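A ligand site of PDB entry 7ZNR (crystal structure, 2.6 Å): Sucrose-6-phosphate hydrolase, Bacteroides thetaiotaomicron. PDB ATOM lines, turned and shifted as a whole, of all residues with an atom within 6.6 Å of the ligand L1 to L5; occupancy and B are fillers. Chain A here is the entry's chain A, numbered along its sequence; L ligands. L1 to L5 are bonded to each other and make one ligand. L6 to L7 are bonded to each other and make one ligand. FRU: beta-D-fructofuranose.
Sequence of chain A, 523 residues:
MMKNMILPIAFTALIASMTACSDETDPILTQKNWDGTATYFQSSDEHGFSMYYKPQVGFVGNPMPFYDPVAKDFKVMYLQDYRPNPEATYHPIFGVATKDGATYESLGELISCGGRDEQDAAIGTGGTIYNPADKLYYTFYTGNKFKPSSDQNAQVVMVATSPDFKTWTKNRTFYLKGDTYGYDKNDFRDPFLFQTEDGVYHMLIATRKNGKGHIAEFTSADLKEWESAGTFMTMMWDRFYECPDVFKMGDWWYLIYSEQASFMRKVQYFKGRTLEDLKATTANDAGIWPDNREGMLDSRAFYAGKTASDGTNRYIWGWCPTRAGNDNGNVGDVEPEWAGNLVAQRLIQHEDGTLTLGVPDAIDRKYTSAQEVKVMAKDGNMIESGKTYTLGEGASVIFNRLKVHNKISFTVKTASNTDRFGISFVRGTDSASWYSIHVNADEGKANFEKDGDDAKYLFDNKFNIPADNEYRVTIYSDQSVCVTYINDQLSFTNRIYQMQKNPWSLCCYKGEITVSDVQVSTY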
ATOM      1  N   LYS A 212     -14.035 -11.006 -19.067  1.00  0.00           N
ATOM      2  CA  LYS A 212     -14.912 -10.354 -20.047  1.00  0.00           C
ATOM      3  C   LYS A 212     -16.174  -9.724 -19.404  1.00  0.00           C
ATOM      4  O   LYS A 212     -16.818 -10.306 -18.535  1.00  0.00           O
ATOM      5  CB  LYS A 212     -15.386 -11.269 -21.179  1.00  0.00           C
ATOM      6  CG  LYS A 212     -16.262 -10.522 -22.198  1.00  0.00           C
ATOM      7  CD  LYS A 212     -16.583 -11.165 -23.545  1.00  0.00           C
ATOM      8  CE  LYS A 212     -15.709 -10.717 -24.711  1.00  0.00           C
ATOM      9  NZ  LYS A 212     -16.199  -9.497 -25.397  1.00  0.00           N
ATOM     10  N   MET A 235     -20.654  -7.816 -23.172  1.00  0.00           N
ATOM     11  CA  MET A 235     -20.145  -6.485 -23.498  1.00  0.00           C
ATOM     12  C   MET A 235     -19.081  -6.641 -24.580  1.00  0.00           C
ATOM     13  O   MET A 235     -18.304  -7.566 -24.582  1.00  0.00           O
ATOM     14  CB  MET A 235     -19.527  -5.815 -22.268  1.00  0.00           C
ATOM     15  CG  MET A 235     -20.581  -5.397 -21.248  1.00  0.00           C
ATOM     16  SD  MET A 235     -19.829  -4.967 -19.681  1.00  0.00           S
ATOM     17  CE  MET A 235     -21.275  -4.880 -18.631  1.00  0.00           C
ATOM     18  N   MET A 236     -19.108  -5.727 -25.540  1.00  0.00           N
ATOM     19  CA  MET A 236     -18.366  -5.915 -26.770  1.00  0.00           C
ATOM     20  C   MET A 236     -16.879  -5.848 -26.426  1.00  0.00           C
ATOM     21  O   MET A 236     -16.481  -5.073 -25.575  1.00  0.00           O
ATOM     22  CB  MET A 236     -18.728  -4.813 -27.747  1.00  0.00           C
ATOM     23  CG  MET A 236     -18.441  -5.195 -29.169  1.00  0.00           C
ATOM     24  SD  MET A 236     -19.764  -6.155 -29.873  1.00  0.00           S
ATOM     25  CE  MET A 236     -21.104  -4.981 -29.652  1.00  0.00           C
ATOM     26  N   TRP A 237     -16.061  -6.679 -27.082  1.00  0.00           N
ATOM     27  CA  TRP A 237     -14.619  -6.605 -26.940  1.00  0.00           C
ATOM     28  C   TRP A 237     -14.263  -6.446 -25.470  1.00  0.00           C
ATOM     29  O   TRP A 237     -14.755  -7.191 -24.641  1.00  0.00           O
ATOM     30  CB  TRP A 237     -14.062  -5.485 -27.835  1.00  0.00           C
ATOM     31  CG  TRP A 237     -14.484  -5.654 -29.256  1.00  0.00           C
ATOM     32  CD1 TRP A 237     -14.352  -6.789 -29.998  1.00  0.00           C
ATOM     33  CD2 TRP A 237     -15.106  -4.675 -30.110  1.00  0.00           C
ATOM     34  NE1 TRP A 237     -14.860  -6.590 -31.252  1.00  0.00           N
ATOM     35  CE2 TRP A 237     -15.314  -5.298 -31.364  1.00  0.00           C
ATOM     36  CE3 TRP A 237     -15.517  -3.350 -29.929  1.00  0.00           C
ATOM     37  CZ2 TRP A 237     -15.901  -4.635 -32.447  1.00  0.00           C
ATOM     38  CZ3 TRP A 237     -16.097  -2.703 -30.998  1.00  0.00           C
ATOM     39  CH2 TRP A 237     -16.283  -3.335 -32.245  1.00  0.00           C
ATOM     40  N   ASP A 238     -13.393  -5.492 -25.140  1.00  0.00           N
ATOM     41  CA  ASP A 238     -12.989  -5.257 -23.753  1.00  0.00           C
ATOM     42  C   ASP A 238     -13.702  -4.025 -23.172  1.00  0.00           C
ATOM     43  O   ASP A 238     -13.272  -3.484 -22.165  1.00  0.00           O
ATOM     44  CB  ASP A 238     -11.465  -5.096 -23.664  1.00  0.00           C
ATOM     45  CG  ASP A 238     -10.895  -4.031 -24.590  1.00  0.00           C
ATOM     46  OD1 ASP A 238     -11.638  -3.457 -25.439  1.00  0.00           O
ATOM     47  OD2 ASP A 238      -9.696  -3.763 -24.471  1.00  0.00           O
ATOM     48  N   ARG A 239     -14.795  -3.583 -23.814  1.00  0.00           N
ATOM     49  CA  ARG A 239     -15.590  -2.490 -23.322  1.00  0.00           C
ATOM     50  C   ARG A 239     -16.201  -2.831 -21.968  1.00  0.00           C
ATOM     51  O   ARG A 239     -16.277  -4.007 -21.608  1.00  0.00           O
ATOM     52  CB  ARG A 239     -16.740  -2.226 -24.289  1.00  0.00           C
ATOM     53  CG  ARG A 239     -16.340  -1.997 -25.753  1.00  0.00           C
ATOM     54  CD  ARG A 239     -15.389  -0.854 -25.946  1.00  0.00           C
ATOM     55  NE  ARG A 239     -15.084  -0.572 -27.348  1.00  0.00           N
ATOM     56  CZ  ARG A 239     -15.827   0.145 -28.165  1.00  0.00           C
ATOM     57  NH1 ARG A 239     -17.041   0.542 -27.842  1.00  0.00           N
ATOM     58  NH2 ARG A 239     -15.325   0.457 -29.342  1.00  0.00           N
ATOM     59  N   ALA A 261     -14.919   2.838 -21.374  1.00  0.00           N
ATOM     60  CA  ALA A 261     -13.687   2.879 -22.142  1.00  0.00           C
ATOM     61  C   ALA A 261     -13.276   4.337 -22.320  1.00  0.00           C
ATOM     62  O   ALA A 261     -14.073   5.194 -22.720  1.00  0.00           O
ATOM     63  CB  ALA A 261     -13.832   2.175 -23.485  1.00  0.00           C
ATOM     64  N   SER A 262     -11.992   4.552 -22.012  1.00  0.00           N
ATOM     65  CA  SER A 262     -11.384   5.847 -21.831  1.00  0.00           C
ATOM     66  C   SER A 262     -11.494   6.704 -23.075  1.00  0.00           C
ATOM     67  O   SER A 262     -11.446   7.910 -23.020  1.00  0.00           O
ATOM     68  CB  SER A 262      -9.933   5.632 -21.528  1.00  0.00           C
ATOM     69  OG  SER A 262      -9.412   6.797 -20.918  1.00  0.00           O
ATOM     70  N   PHE A 263     -11.507   6.067 -24.231  1.00  0.00           N
ATOM     71  CA  PHE A 263     -11.533   6.783 -25.493  1.00  0.00           C
ATOM     72  C   PHE A 263     -12.966   7.105 -25.886  1.00  0.00           C
ATOM     73  O   PHE A 263     -13.174   7.763 -26.875  1.00  0.00           O
ATOM     74  CB  PHE A 263     -10.851   5.958 -26.593  1.00  0.00           C
ATOM     75  CG  PHE A 263     -11.414   4.571 -26.788  1.00  0.00           C
ATOM     76  CD1 PHE A 263     -12.655   4.403 -27.412  1.00  0.00           C
ATOM     77  CD2 PHE A 263     -10.737   3.455 -26.281  1.00  0.00           C
ATOM     78  CE1 PHE A 263     -13.182   3.135 -27.564  1.00  0.00           C
ATOM     79  CE2 PHE A 263     -11.288   2.199 -26.416  1.00  0.00           C
ATOM     80  CZ  PHE A 263     -12.506   2.036 -27.059  1.00  0.00           C
ATOM     81  N   MET A 264     -13.960   6.632 -25.134  1.00  0.00           N
ATOM     82  CA  MET A 264     -15.327   6.817 -25.601  1.00  0.00           C
ATOM     83  C   MET A 264     -16.039   7.768 -24.650  1.00  0.00           C
ATOM     84  O   MET A 264     -16.208   8.948 -24.954  1.00  0.00           O
ATOM     85  CB  MET A 264     -16.015   5.454 -25.763  1.00  0.00           C
ATOM     86  CG  MET A 264     -17.464   5.531 -26.245  1.00  0.00           C
ATOM     87  SD  MET A 264     -17.702   5.881 -28.029  1.00  0.00           S
ATOM     88  CE  MET A 264     -17.431   4.226 -28.676  1.00  0.00           C
ATOM     89  N   GLN A 268     -24.352   5.312 -25.208  1.00  0.00           N
ATOM     90  CA  GLN A 268     -24.645   4.592 -26.436  1.00  0.00           C
ATOM     91  C   GLN A 268     -25.927   3.767 -26.291  1.00  0.00           C
ATOM     92  O   GLN A 268     -26.562   3.771 -25.250  1.00  0.00           O
ATOM     93  CB  GLN A 268     -23.451   3.717 -26.792  1.00  0.00           C
ATOM     94  CG  GLN A 268     -22.135   4.459 -26.925  1.00  0.00           C
ATOM     95  CD  GLN A 268     -21.079   3.494 -27.446  1.00  0.00           C
ATOM     96  OE1 GLN A 268     -20.203   3.028 -26.719  1.00  0.00           O
ATOM     97  NE2 GLN A 268     -21.209   3.137 -28.725  1.00  0.00           N
ATOM     98  N   ASP A 285     -19.214 -10.812 -30.012  1.00  0.00           N
ATOM     99  CA  ASP A 285     -18.680  -9.557 -30.504  1.00  0.00           C
ATOM    100  C   ASP A 285     -19.259  -9.329 -31.903  1.00  0.00           C
ATOM    101  O   ASP A 285     -18.536  -8.968 -32.823  1.00  0.00           O
ATOM    102  CB  ASP A 285     -17.150  -9.491 -30.387  1.00  0.00           C
ATOM    103  CG  ASP A 285     -16.656  -9.671 -28.962  1.00  0.00           C
ATOM    104  OD1 ASP A 285     -17.509  -9.609 -28.031  1.00  0.00           O
ATOM    105  OD2 ASP A 285     -15.426  -9.888 -28.765  1.00  0.00           O
ATOM    106  N   TRP A 289     -24.543  -2.622 -34.525  1.00  0.00           N
ATOM    107  CA  TRP A 289     -24.866  -1.243 -34.143  1.00  0.00           C
ATOM    108  C   TRP A 289     -26.242  -0.901 -34.662  1.00  0.00           C
ATOM    109  O   TRP A 289     -26.597  -1.361 -35.727  1.00  0.00           O
ATOM    110  CB  TRP A 289     -23.878  -0.237 -34.730  1.00  0.00           C
ATOM    111  CG  TRP A 289     -22.468  -0.654 -34.525  1.00  0.00           C
ATOM    112  CD1 TRP A 289     -21.579  -1.009 -35.491  1.00  0.00           C
ATOM    113  CD2 TRP A 289     -21.820  -0.841 -33.261  1.00  0.00           C
ATOM    114  NE1 TRP A 289     -20.396  -1.387 -34.903  1.00  0.00           N
ATOM    115  CE2 TRP A 289     -20.524  -1.308 -33.542  1.00  0.00           C
ATOM    116  CE3 TRP A 289     -22.184  -0.646 -31.930  1.00  0.00           C
ATOM    117  CZ2 TRP A 289     -19.577  -1.545 -32.551  1.00  0.00           C
ATOM    118  CZ3 TRP A 289     -21.253  -0.872 -30.934  1.00  0.00           C
ATOM    119  CH2 TRP A 289     -19.966  -1.302 -31.240  1.00  0.00           C
ATOM    120  N   GLU A 294     -22.723   3.916 -34.429  1.00  0.00           N
ATOM    121  CA  GLU A 294     -22.417   3.076 -33.276  1.00  0.00           C
ATOM    122  C   GLU A 294     -23.400   3.329 -32.129  1.00  0.00           C
ATOM    123  O   GLU A 294     -23.150   2.968 -30.977  1.00  0.00           O
ATOM    124  CB  GLU A 294     -20.953   3.262 -32.844  1.00  0.00           C
ATOM    125  CG  GLU A 294     -19.889   2.790 -33.837  1.00  0.00           C
ATOM    126  CD  GLU A 294     -18.472   2.762 -33.261  1.00  0.00           C
ATOM    127  OE1 GLU A 294     -18.037   3.736 -32.587  1.00  0.00           O
ATOM    128  OE2 GLU A 294     -17.774   1.775 -33.492  1.00  0.00           O
ATOM    129  N   MET A 296     -23.994   6.089 -30.713  1.00  0.00           N
ATOM    130  CA  MET A 296     -23.582   7.238 -29.921  1.00  0.00           C
ATOM    131  C   MET A 296     -24.620   8.342 -29.995  1.00  0.00           C
ATOM    132  O   MET A 296     -24.758   8.912 -31.076  1.00  0.00           O
ATOM    133  CB  MET A 296     -22.270   7.816 -30.439  1.00  0.00           C
ATOM    134  CG  MET A 296     -21.133   6.918 -30.080  1.00  0.00           C
ATOM    135  SD  MET A 296     -19.633   7.168 -30.979  1.00  0.00           S
ATOM    136  CE  MET A 296     -20.177   7.723 -32.599  1.00  0.00           C
HETATM  137  C1  FRU L   1     -12.140  -9.512 -26.026  1.00  0.00           C
HETATM  138  C2  FRU L   1     -11.094  -9.185 -27.153  1.00  0.00           C
HETATM  139  C3  FRU L   1     -10.519  -7.753 -26.978  1.00  0.00           C
HETATM  140  C4  FRU L   1      -9.938  -7.398 -28.336  1.00  0.00           C
HETATM  141  C5  FRU L   1     -10.927  -8.073 -29.311  1.00  0.00           C
HETATM  142  C6  FRU L   1     -10.387  -8.544 -30.676  1.00  0.00           C
HETATM  143  O1  FRU L   1     -13.243 -10.388 -26.373  1.00  0.00           O
HETATM  144  O2  FRU L   1     -10.078 -10.200 -27.098  1.00  0.00           O
HETATM  145  O3  FRU L   1      -9.578  -7.578 -25.899  1.00  0.00           O
HETATM  146  O4  FRU L   1      -9.851  -5.973 -28.423  1.00  0.00           O
HETATM  147  O5  FRU L   1     -11.528  -9.154 -28.543  1.00  0.00           O
HETATM  148  O6  FRU L   1     -10.694  -7.580 -31.761  1.00  0.00           O
HETATM  149  C1  FRU L   2     -10.571  -8.055 -33.511  1.00  0.00           C
HETATM  150  C2  FRU L   2     -10.765  -6.601 -32.892  1.00  0.00           C
HETATM  151  C3  FRU L   2     -11.310  -5.432 -33.766  1.00  0.00           C
HETATM  152  C4  FRU L   2     -11.337  -4.314 -32.747  1.00  0.00           C
HETATM  153  C5  FRU L   2      -9.868  -4.342 -32.307  1.00  0.00           C
HETATM  154  C6  FRU L   2      -9.412  -3.730 -30.918  1.00  0.00           C
HETATM  155  O1  FRU L   2     -10.663  -8.246 -34.937  1.00  0.00           O
HETATM  156  O3  FRU L   2     -12.641  -5.372 -34.279  1.00  0.00           O
HETATM  157  O4  FRU L   2     -11.936  -3.184 -33.382  1.00  0.00           O
HETATM  158  O5  FRU L   2      -9.622  -5.808 -32.384  1.00  0.00           O
HETATM  159  O6  FRU L   2     -10.026  -2.506 -30.329  1.00  0.00           O
HETATM  160  C1  FRU L   3      -9.371  -1.515 -28.104  1.00  0.00           C
HETATM  161  C2  FRU L   3     -10.244  -1.376 -29.329  1.00  0.00           C
HETATM  162  C3  FRU L   3     -11.713  -1.883 -29.127  1.00  0.00           C
HETATM  163  C4  FRU L   3     -12.320  -0.948 -30.164  1.00  0.00           C
HETATM  164  C5  FRU L   3     -11.286   0.103 -30.646  1.00  0.00           C
HETATM  165  C6  FRU L   3     -11.814   1.477 -31.044  1.00  0.00           C
HETATM  166  O1  FRU L   3      -8.183  -2.099 -28.654  1.00  0.00           O
HETATM  167  O3  FRU L   3     -12.357  -1.980 -27.812  1.00  0.00           O
HETATM  168  O4  FRU L   3     -12.466  -1.932 -31.216  1.00  0.00           O
HETATM  169  O5  FRU L   3     -10.220   0.065 -29.682  1.00  0.00           O
HETATM  170  O6  FRU L   3     -12.769   1.426 -32.192  1.00  0.00           O
HETATM  171  C1  FRU L   4     -13.431   2.410 -34.434  1.00  0.00           C
HETATM  172  C2  FRU L   4     -13.289   2.548 -32.943  1.00  0.00           C
HETATM  173  C3  FRU L   4     -14.561   3.181 -32.367  1.00  0.00           C
HETATM  174  C4  FRU L   4     -14.043   4.153 -31.329  1.00  0.00           C
HETATM  175  C5  FRU L   4     -12.778   4.652 -31.994  1.00  0.00           C
HETATM  176  C6  FRU L   4     -11.669   5.130 -31.077  1.00  0.00           C
HETATM  177  O1  FRU L   4     -14.296   1.289 -34.500  1.00  0.00           O
HETATM  178  O3  FRU L   4     -15.455   2.258 -31.791  1.00  0.00           O
HETATM  179  O4  FRU L   4     -15.001   5.199 -31.115  1.00  0.00           O
HETATM  180  O5  FRU L   4     -12.285   3.549 -32.758  1.00  0.00           O
HETATM  181  O6  FRU L   4     -10.582   5.651 -31.882  1.00  0.00           O
HETATM  182  C1  FRU L   5      -8.515   7.431 -32.952  1.00  0.00           C
HETATM  183  C2  FRU L   5      -9.607   6.709 -32.121  1.00  0.00           C
HETATM  184  C3  FRU L   5      -9.844   7.642 -30.898  1.00  0.00           C
HETATM  185  C4  FRU L   5      -9.380   6.786 -29.740  1.00  0.00           C
HETATM  186  C5  FRU L   5      -8.438   5.741 -30.375  1.00  0.00           C
HETATM  187  C6  FRU L   5      -8.253   4.443 -29.599  1.00  0.00           C
HETATM  188  O1  FRU L   5      -8.553   7.080 -34.340  1.00  0.00           O
HETATM  189  O3  FRU L   5     -11.164   8.218 -30.719  1.00  0.00           O
HETATM  190  O4  FRU L   5      -8.748   7.648 -28.771  1.00  0.00           O
HETATM  191  O5  FRU L   5      -8.995   5.477 -31.667  1.00  0.00           O
HETATM  192  O6  FRU L   5      -6.840   4.126 -29.682  1.00  0.00           O
HETATM  193  C1  FRU L   6     -12.551   9.117 -33.770  1.00  0.00           C
HETATM  194  C2  FRU L   6     -12.653  10.508 -34.403  1.00  0.00           C
HETATM  195  C3  FRU L   6     -13.152  10.423 -35.847  1.00  0.00           C
HETATM  196  C4  FRU L   6     -12.177  11.238 -36.652  1.00  0.00           C
HETATM  197  C5  FRU L   6     -11.241  11.976 -35.597  1.00  0.00           C
HETATM  198  C6  FRU L   6     -11.454  13.506 -35.347  1.00  0.00           C
HETATM  199  O1  FRU L   6     -11.221   8.621 -33.872  1.00  0.00           O
HETATM  200  O2  FRU L   6     -13.696  11.162 -33.664  1.00  0.00           O
HETATM  201  O3  FRU L   6     -14.457  10.982 -36.007  1.00  0.00           O
HETATM  202  O4  FRU L   6     -11.627  10.294 -37.636  1.00  0.00           O
HETATM  203  O5  FRU L   6     -11.407  11.329 -34.323  1.00  0.00           O
HETATM  204  O6  FRU L   6     -11.011  14.420 -36.425  1.00  0.00           O
HETATM  205  C1  FRU L   7      -9.054  14.864 -38.294  1.00  0.00           C
HETATM  206  C2  FRU L   7      -9.865  15.164 -37.015  1.00  0.00           C
HETATM  207  C3  FRU L   7     -10.544  16.538 -37.165  1.00  0.00           C
HETATM  208  C4  FRU L   7     -10.004  17.329 -35.996  1.00  0.00           C
HETATM  209  C5  FRU L   7      -8.539  16.766 -35.779  1.00  0.00           C
HETATM  210  C6  FRU L   7      -7.856  16.557 -34.379  1.00  0.00           C
HETATM  211  O1  FRU L   7      -9.957  14.990 -39.367  1.00  0.00           O
HETATM  212  O3  FRU L   7     -11.992  16.585 -37.276  1.00  0.00           O
HETATM  213  O4  FRU L   7     -10.301  18.650 -36.499  1.00  0.00           O
HETATM  214  O5  FRU L   7      -8.693  15.407 -36.203  1.00  0.00           O
HETATM  215  O6  FRU L   7      -6.413  16.450 -34.335  1.00  0.00           O
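An oxygen (O3) of FRU L4 lies within hydrogen-bond range of the side-chain carboxylate (OE2) of Glu 294, at 2.9 Å. The side-chain carboxylate (OD2) of Asp 285 lies within hydrogen-bond range of an oxygen (O1) of FRU L1 (3.3 Å). An oxygen (O3) of FRU L4 lies within hydrogen-bond range of the guanidinium group (NH2) of Arg 239 (3.0 Å). OD1 of Asp 238 is in hydrogen-bond range of O3 of FRU L3 (2.9 Å). NZ of Lys 212 lies close to O1 of FRU L1 (3.2 Å).
An oxygen (O1) of FRU L6 lies close to an oxygen (O1) of FRU L5.
The side-chain amino group (NZ) of Lys 212 lies within hydrogen-bond range of the backbone carbonyl oxygen (O) of Met 235, 3.0 Å away. NZ of Lys 212 lies within hydrogen-bond range of O of Trp 237 (2.8 Å). The side-chain carboxylate (OD1) of Asp 285 lies within salt-bridge range of the side-chain amino group (NZ) of Lys 212 (2.9 Å). NE2 of Gln 268 sits at hydrogen-bond distance from O of Glu 294 (3.0 Å). OD1 of Asp 285 is in hydrogen-bond range of N of Trp 237 (3.4 Å).
CE3 of Trp 237 touches O4 of FRU L3, 3.6 Å away. CB of Phe 263 touches O4 of FRU L5 (3.5 Å). CE of Met 264 touches O4 of FRU L4 (3.6 Å). Hydrophobic or aromatic side chains that line the ligand L1 to L5: Trp 237, Phe 263 and Met 264. Within 4 Å of the ligand L1 to L5: Lys 212, Trp 237, Asp 238, Arg 239, Phe 263, Met 264, Asp 285 and Glu 294. The nearest printed residue that does not touch the ligand L1 to L5 is Met 296 (5.0 Å).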
